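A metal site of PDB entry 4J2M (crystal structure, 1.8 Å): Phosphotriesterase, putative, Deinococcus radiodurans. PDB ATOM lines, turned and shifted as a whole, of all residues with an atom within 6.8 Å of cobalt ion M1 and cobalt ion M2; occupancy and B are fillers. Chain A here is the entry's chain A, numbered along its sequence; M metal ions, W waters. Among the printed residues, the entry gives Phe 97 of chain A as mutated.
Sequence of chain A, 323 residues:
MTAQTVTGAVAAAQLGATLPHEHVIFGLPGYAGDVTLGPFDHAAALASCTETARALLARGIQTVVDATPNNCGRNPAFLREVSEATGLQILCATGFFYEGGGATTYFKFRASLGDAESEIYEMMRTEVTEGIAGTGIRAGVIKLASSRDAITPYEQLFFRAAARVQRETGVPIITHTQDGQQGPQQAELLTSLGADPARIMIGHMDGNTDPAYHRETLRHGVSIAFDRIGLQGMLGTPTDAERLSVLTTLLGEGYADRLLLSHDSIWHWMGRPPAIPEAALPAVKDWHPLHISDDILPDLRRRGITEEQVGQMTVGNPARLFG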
ATOM      1  N   HIS A  21      -7.988  23.639  33.407  1.00  0.00           N
ATOM      2  CA  HIS A  21      -6.930  22.813  32.808  1.00  0.00           C
ATOM      3  C   HIS A  21      -6.054  22.231  33.936  1.00  0.00           C
ATOM      4  O   HIS A  21      -5.143  22.892  34.430  1.00  0.00           O
ATOM      5  CB  HIS A  21      -6.054  23.596  31.846  1.00  0.00           C
ATOM      6  CG  HIS A  21      -5.057  22.745  31.091  1.00  0.00           C
ATOM      7  ND1 HIS A  21      -5.004  22.698  29.712  1.00  0.00           N
ATOM      8  CD2 HIS A  21      -4.111  21.887  31.540  1.00  0.00           C
ATOM      9  CE1 HIS A  21      -4.035  21.866  29.339  1.00  0.00           C
ATOM     10  NE2 HIS A  21      -3.480  21.360  30.421  1.00  0.00           N
ATOM     11  N   GLU A  22      -6.356  20.993  34.290  1.00  0.00           N
ATOM     12  CA  GLU A  22      -5.582  20.246  35.292  1.00  0.00           C
ATOM     13  C   GLU A  22      -5.498  18.774  34.880  1.00  0.00           C
ATOM     14  O   GLU A  22      -6.193  18.303  33.971  1.00  0.00           O
ATOM     15  CB  GLU A  22      -6.251  20.322  36.672  1.00  0.00           C
ATOM     16  CG  GLU A  22      -6.664  21.726  37.134  1.00  0.00           C
ATOM     17  CD  GLU A  22      -5.472  22.596  37.501  1.00  0.00           C
ATOM     18  OE1 GLU A  22      -4.393  22.021  37.841  1.00  0.00           O
ATOM     19  OE2 GLU A  22      -5.610  23.842  37.460  1.00  0.00           O
ATOM     20  N   HIS A  23      -4.653  18.033  35.593  1.00  0.00           N
ATOM     21  CA  HIS A  23      -4.524  16.613  35.341  1.00  0.00           C
ATOM     22  C   HIS A  23      -4.667  15.828  36.652  1.00  0.00           C
ATOM     23  O   HIS A  23      -3.770  15.839  37.496  1.00  0.00           O
ATOM     24  CB  HIS A  23      -3.174  16.356  34.662  1.00  0.00           C
ATOM     25  CG  HIS A  23      -3.004  17.057  33.346  1.00  0.00           C
ATOM     26  ND1 HIS A  23      -3.570  16.580  32.181  1.00  0.00           N
ATOM     27  CD2 HIS A  23      -2.328  18.184  32.995  1.00  0.00           C
ATOM     28  CE1 HIS A  23      -3.277  17.385  31.173  1.00  0.00           C
ATOM     29  NE2 HIS A  23      -2.512  18.359  31.639  1.00  0.00           N
ATOM     30  N   PHE A  26      -1.760  11.574  35.239  1.00  0.00           N
ATOM     31  CA  PHE A  26      -1.054  11.892  34.009  1.00  0.00           C
ATOM     32  C   PHE A  26       0.171  11.048  33.872  1.00  0.00           C
ATOM     33  O   PHE A  26       0.978  10.990  34.799  1.00  0.00           O
ATOM     34  CB  PHE A  26      -0.596  13.344  34.003  1.00  0.00           C
ATOM     35  CG  PHE A  26      -0.047  13.825  32.683  1.00  0.00           C
ATOM     36  CD1 PHE A  26      -0.890  14.384  31.726  1.00  0.00           C
ATOM     37  CD2 PHE A  26       1.302  13.740  32.411  1.00  0.00           C
ATOM     38  CE1 PHE A  26      -0.381  14.832  30.497  1.00  0.00           C
ATOM     39  CE2 PHE A  26       1.818  14.199  31.194  1.00  0.00           C
ATOM     40  CZ  PHE A  26       0.962  14.739  30.234  1.00  0.00           C
ATOM     41  N   ALA A  67      -7.632  17.836  31.340  1.00  0.00           N
ATOM     42  CA  ALA A  67      -7.209  18.051  29.966  1.00  0.00           C
ATOM     43  C   ALA A  67      -6.339  16.908  29.437  1.00  0.00           C
ATOM     44  O   ALA A  67      -5.707  17.054  28.404  1.00  0.00           O
ATOM     45  CB  ALA A  67      -6.451  19.307  29.902  1.00  0.00           C
ATOM     46  N   THR A  68      -6.328  15.779  30.140  1.00  0.00           N
ATOM     47  CA  THR A  68      -5.407  14.667  29.817  1.00  0.00           C
ATOM     48  C   THR A  68      -5.715  14.018  28.461  1.00  0.00           C
ATOM     49  O   THR A  68      -6.777  13.414  28.293  1.00  0.00           O
ATOM     50  CB  THR A  68      -5.450  13.582  30.920  1.00  0.00           C
ATOM     51  OG1 THR A  68      -5.184  14.188  32.196  1.00  0.00           O
ATOM     52  CG2 THR A  68      -4.405  12.490  30.663  1.00  0.00           C
ATOM     53  N   PRO A  69      -4.770  14.089  27.510  1.00  0.00           N
ATOM     54  CA  PRO A  69      -5.039  13.444  26.210  1.00  0.00           C
ATOM     55  C   PRO A  69      -5.102  11.893  26.263  1.00  0.00           C
ATOM     56  O   PRO A  69      -4.601  11.278  27.212  1.00  0.00           O
ATOM     57  CB  PRO A  69      -3.866  13.907  25.325  1.00  0.00           C
ATOM     58  CG  PRO A  69      -3.229  15.041  26.046  1.00  0.00           C
ATOM     59  CD  PRO A  69      -3.480  14.791  27.517  1.00  0.00           C
ATOM     60  N   PHE A  97      -1.829  14.173  21.917  1.00  0.00           N
ATOM     61  CA  PHE A  97      -0.885  15.232  22.244  1.00  0.00           C
ATOM     62  C   PHE A  97       0.132  15.652  21.094  1.00  0.00           C
ATOM     63  O   PHE A  97       0.419  14.827  20.225  1.00  0.00           O
ATOM     64  CB  PHE A  97      -0.199  14.785  23.560  1.00  0.00           C
ATOM     65  CG  PHE A  97       1.022  15.488  23.801  1.00  0.00           C
ATOM     66  CD1 PHE A  97       1.010  16.800  23.553  1.00  0.00           C
ATOM     67  CD2 PHE A  97       2.166  14.886  24.255  1.00  0.00           C
ATOM     68  CE1 PHE A  97       2.079  17.543  23.703  1.00  0.00           C
ATOM     69  CE2 PHE A  97       3.298  15.627  24.428  1.00  0.00           C
ATOM     70  CZ  PHE A  97       3.249  16.973  24.149  1.00  0.00           C
ATOM     71  N   KCX A 143      -9.342  18.156  23.320  1.00  0.00           N
ATOM     72  CA  KCX A 143      -7.976  18.543  23.567  1.00  0.00           C
ATOM     73  CB  KCX A 143      -7.298  17.634  24.609  1.00  0.00           C
ATOM     74  CG  KCX A 143      -6.401  18.388  25.597  1.00  0.00           C
ATOM     75  CD  KCX A 143      -5.276  19.120  24.913  1.00  0.00           C
ATOM     76  CE  KCX A 143      -4.320  19.845  25.849  1.00  0.00           C
ATOM     77  NZ  KCX A 143      -3.859  19.097  27.098  1.00  0.00           N
ATOM     78  C   KCX A 143      -7.167  18.566  22.287  1.00  0.00           C
ATOM     79  O   KCX A 143      -7.002  17.535  21.629  1.00  0.00           O
ATOM     80  CX  KCX A 143      -2.743  19.394  27.773  1.00  0.00           C
ATOM     81  OQ1 KCX A 143      -2.526  18.761  28.819  1.00  0.00           O
ATOM     82  OQ2 KCX A 143      -1.942  20.251  27.395  1.00  0.00           O
ATOM     83  N   ALA A 145      -3.321  20.034  20.497  1.00  0.00           N
ATOM     84  CA  ALA A 145      -1.984  20.469  20.838  1.00  0.00           C
ATOM     85  C   ALA A 145      -1.191  20.713  19.575  1.00  0.00           C
ATOM     86  O   ALA A 145      -1.383  20.018  18.588  1.00  0.00           O
ATOM     87  CB  ALA A 145      -1.309  19.412  21.682  1.00  0.00           C
ATOM     88  N   THR A 175      -6.784  23.890  24.262  1.00  0.00           N
ATOM     89  CA  THR A 175      -5.545  23.566  23.595  1.00  0.00           C
ATOM     90  C   THR A 175      -4.303  23.651  24.464  1.00  0.00           C
ATOM     91  O   THR A 175      -4.314  24.272  25.547  1.00  0.00           O
ATOM     92  CB  THR A 175      -5.264  24.489  22.378  1.00  0.00           C
ATOM     93  OG1 THR A 175      -4.668  25.716  22.812  1.00  0.00           O
ATOM     94  CG2 THR A 175      -6.530  24.752  21.609  1.00  0.00           C
ATOM     95  N   HIS A 176      -3.244  23.011  23.943  1.00  0.00           N
ATOM     96  CA  HIS A 176      -1.872  23.120  24.411  1.00  0.00           C
ATOM     97  C   HIS A 176      -1.053  23.931  23.410  1.00  0.00           C
ATOM     98  O   HIS A 176      -1.051  23.615  22.218  1.00  0.00           O
ATOM     99  CB  HIS A 176      -1.296  21.687  24.519  1.00  0.00           C
ATOM    100  CG  HIS A 176       0.180  21.617  24.744  1.00  0.00           C
ATOM    101  ND1 HIS A 176       0.724  21.191  25.947  1.00  0.00           N
ATOM    102  CD2 HIS A 176       1.230  21.850  23.927  1.00  0.00           C
ATOM    103  CE1 HIS A 176       2.037  21.199  25.864  1.00  0.00           C
ATOM    104  NE2 HIS A 176       2.378  21.598  24.650  1.00  0.00           N
ATOM    105  N   THR A 177      -0.332  24.936  23.868  1.00  0.00           N
ATOM    106  CA  THR A 177       0.658  25.592  23.024  1.00  0.00           C
ATOM    107  C   THR A 177       1.999  25.292  23.633  1.00  0.00           C
ATOM    108  O   THR A 177       2.113  25.228  24.851  1.00  0.00           O
ATOM    109  CB  THR A 177       0.488  27.146  22.892  1.00  0.00           C
ATOM    110  OG1 THR A 177       0.556  27.789  24.179  1.00  0.00           O
ATOM    111  CG2 THR A 177      -0.805  27.499  22.164  1.00  0.00           C
ATOM    112  N   GLN A 178       3.007  25.121  22.774  1.00  0.00           N
ATOM    113  CA  GLN A 178       4.352  24.720  23.178  1.00  0.00           C
ATOM    114  C   GLN A 178       5.274  25.937  23.213  1.00  0.00           C
ATOM    115  O   GLN A 178       5.362  26.658  22.220  1.00  0.00           O
ATOM    116  CB  GLN A 178       4.895  23.681  22.171  1.00  0.00           C
ATOM    117  CG  GLN A 178       6.243  23.075  22.535  1.00  0.00           C
ATOM    118  CD  GLN A 178       6.227  22.273  23.842  1.00  0.00           C
ATOM    119  OE1 GLN A 178       5.211  21.668  24.191  1.00  0.00           O
ATOM    120  NE2 GLN A 178       7.348  22.256  24.547  1.00  0.00           N
ATOM    121  N   HIS A 204      -2.011  27.500  27.653  1.00  0.00           N
ATOM    122  CA  HIS A 204      -0.624  27.809  27.976  1.00  0.00           C
ATOM    123  C   HIS A 204      -0.173  29.176  27.441  1.00  0.00           C
ATOM    124  O   HIS A 204       0.988  29.361  27.060  1.00  0.00           O
ATOM    125  CB  HIS A 204       0.345  26.706  27.496  1.00  0.00           C
ATOM    126  CG  HIS A 204      -0.058  25.312  27.895  1.00  0.00           C
ATOM    127  ND1 HIS A 204      -0.814  25.035  28.999  1.00  0.00           N
ATOM    128  CD2 HIS A 204       0.216  24.114  27.308  1.00  0.00           C
ATOM    129  CE1 HIS A 204      -1.010  23.729  29.095  1.00  0.00           C
ATOM    130  NE2 HIS A 204      -0.408  23.150  28.067  1.00  0.00           N
ATOM    131  N   ASP A 227      -2.648  28.997  32.258  1.00  0.00           N
ATOM    132  CA  ASP A 227      -3.027  27.738  32.875  1.00  0.00           C
ATOM    133  C   ASP A 227      -1.849  26.897  33.387  1.00  0.00           C
ATOM    134  O   ASP A 227      -2.047  25.736  33.725  1.00  0.00           O
ATOM    135  CB  ASP A 227      -3.932  26.898  31.969  1.00  0.00           C
ATOM    136  CG  ASP A 227      -3.339  26.677  30.595  1.00  0.00           C
ATOM    137  OD1 ASP A 227      -2.131  26.922  30.431  1.00  0.00           O
ATOM    138  OD2 ASP A 227      -4.100  26.297  29.685  1.00  0.00           O
ATOM    139  N   ARG A 228      -0.668  27.493  33.526  1.00  0.00           N
ATOM    140  CA  ARG A 228       0.439  26.795  34.191  1.00  0.00           C
ATOM    141  C   ARG A 228       0.946  27.625  35.368  1.00  0.00           C
ATOM    142  O   ARG A 228       2.131  27.647  35.688  1.00  0.00           O
ATOM    143  CB  ARG A 228       1.564  26.505  33.206  1.00  0.00           C
ATOM    144  CG  ARG A 228       1.025  25.744  32.009  1.00  0.00           C
ATOM    145  CD  ARG A 228       2.076  25.404  31.042  1.00  0.00           C
ATOM    146  NE  ARG A 228       2.529  24.040  31.271  1.00  0.00           N
ATOM    147  CZ  ARG A 228       3.435  23.438  30.524  1.00  0.00           C
ATOM    148  NH1 ARG A 228       3.969  24.074  29.488  1.00  0.00           N
ATOM    149  NH2 ARG A 228       3.799  22.195  30.815  1.00  0.00           N
ATOM    150  N   ASP A 264      -2.337  23.454  35.491  1.00  0.00           N
ATOM    151  CA  ASP A 264      -1.781  22.339  34.708  1.00  0.00           C
ATOM    152  C   ASP A 264      -1.072  21.384  35.679  1.00  0.00           C
ATOM    153  O   ASP A 264      -0.024  20.801  35.370  1.00  0.00           O
ATOM    154  CB  ASP A 264      -0.782  22.844  33.662  1.00  0.00           C
ATOM    155  CG  ASP A 264      -0.544  21.835  32.499  1.00  0.00           C
ATOM    156  OD1 ASP A 264      -1.333  20.889  32.284  1.00  0.00           O
ATOM    157  OD2 ASP A 264       0.442  22.031  31.756  1.00  0.00           O
ATOM    158  N   SER A 265      -1.656  21.224  36.858  1.00  0.00           N
ATOM    159  CA  SER A 265      -1.042  20.402  37.907  1.00  0.00           C
ATOM    160  C   SER A 265      -1.274  18.914  37.626  1.00  0.00           C
ATOM    161  O   SER A 265      -2.178  18.544  36.878  1.00  0.00           O
ATOM    162  CB  SER A 265      -1.597  20.830  39.288  1.00  0.00           C
ATOM    163  OG  SER A 265      -2.966  20.512  39.400  1.00  0.00           O
HETATM  164 CO    CO M   1      -1.962  19.882  30.516  1.00  0.00          CO
HETATM  165 CO    CO M   2      -0.264  21.105  27.819  1.00  0.00          CO
HETATM  166  O   HOH W   1      -0.357  20.441  29.824  1.00  0.00           O
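NZ of KCX 143 sits at hydrogen-bond distance from the backbone carbonyl oxygen (O) of Ala 67. A ring nitrogen (ND1) of His 23 lies within hydrogen-bond range of the side-chain hydroxyl of Thr 68 (2.9 Å). The backbone carbonyl oxygen (O) of His 204 lies within hydrogen-bond range of the side-chain hydroxyl (OG1) of Thr 177 (3.3 Å). OD1 of Asp 227 sits at hydrogen-bond distance from ND1 of His 204 (2.7 Å). The side-chain amide oxygen (OE1) of Gln 178 sits at hydrogen-bond distance from a ring nitrogen (NE2) of His 176 (2.9 Å). The guanidinium group (NE) of Arg 228 is in salt-bridge range of the side-chain carboxylate (OD2) of Asp 264, at 2.9 Å. The backbone NH of Asp 264 lies within hydrogen-bond range of the side-chain carboxylate of Glu 22, at 3.4 Å. The backbone carbonyl oxygen (O) of Asp 227 lies within hydrogen-bond range of the backbone NH (N) of Asp 264 (2.9 Å).
Of the 19 residues printed, 4 come within 4 Å of cobalt ion M1. The nearest printed residue that does not touch cobalt ion M1 is His 204 (4.2 Å).
The nearest printed residue that does not touch cobalt ion M2 is Asp 264 (4.1 Å).
Cobalt ion M2 is bound by OQ2 of KCX 143 (1.9 Å), NE2 of His 204 (2.1 Å), water W1 (2.1 Å) and ND1 of His 176 (2.1 Å).
Water W1 binds cobalt ion M1. Cobalt ion M1 is bound by a ring nitrogen (NE2) of His 23. Cobalt ion M1 is bound by OQ1 of KCX 143, at 2.1 Å. NE2 of His 21 is bound to cobalt ion M1, 2.1 Å away. OD1 of Asp 264 is bound to cobalt ion M1.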
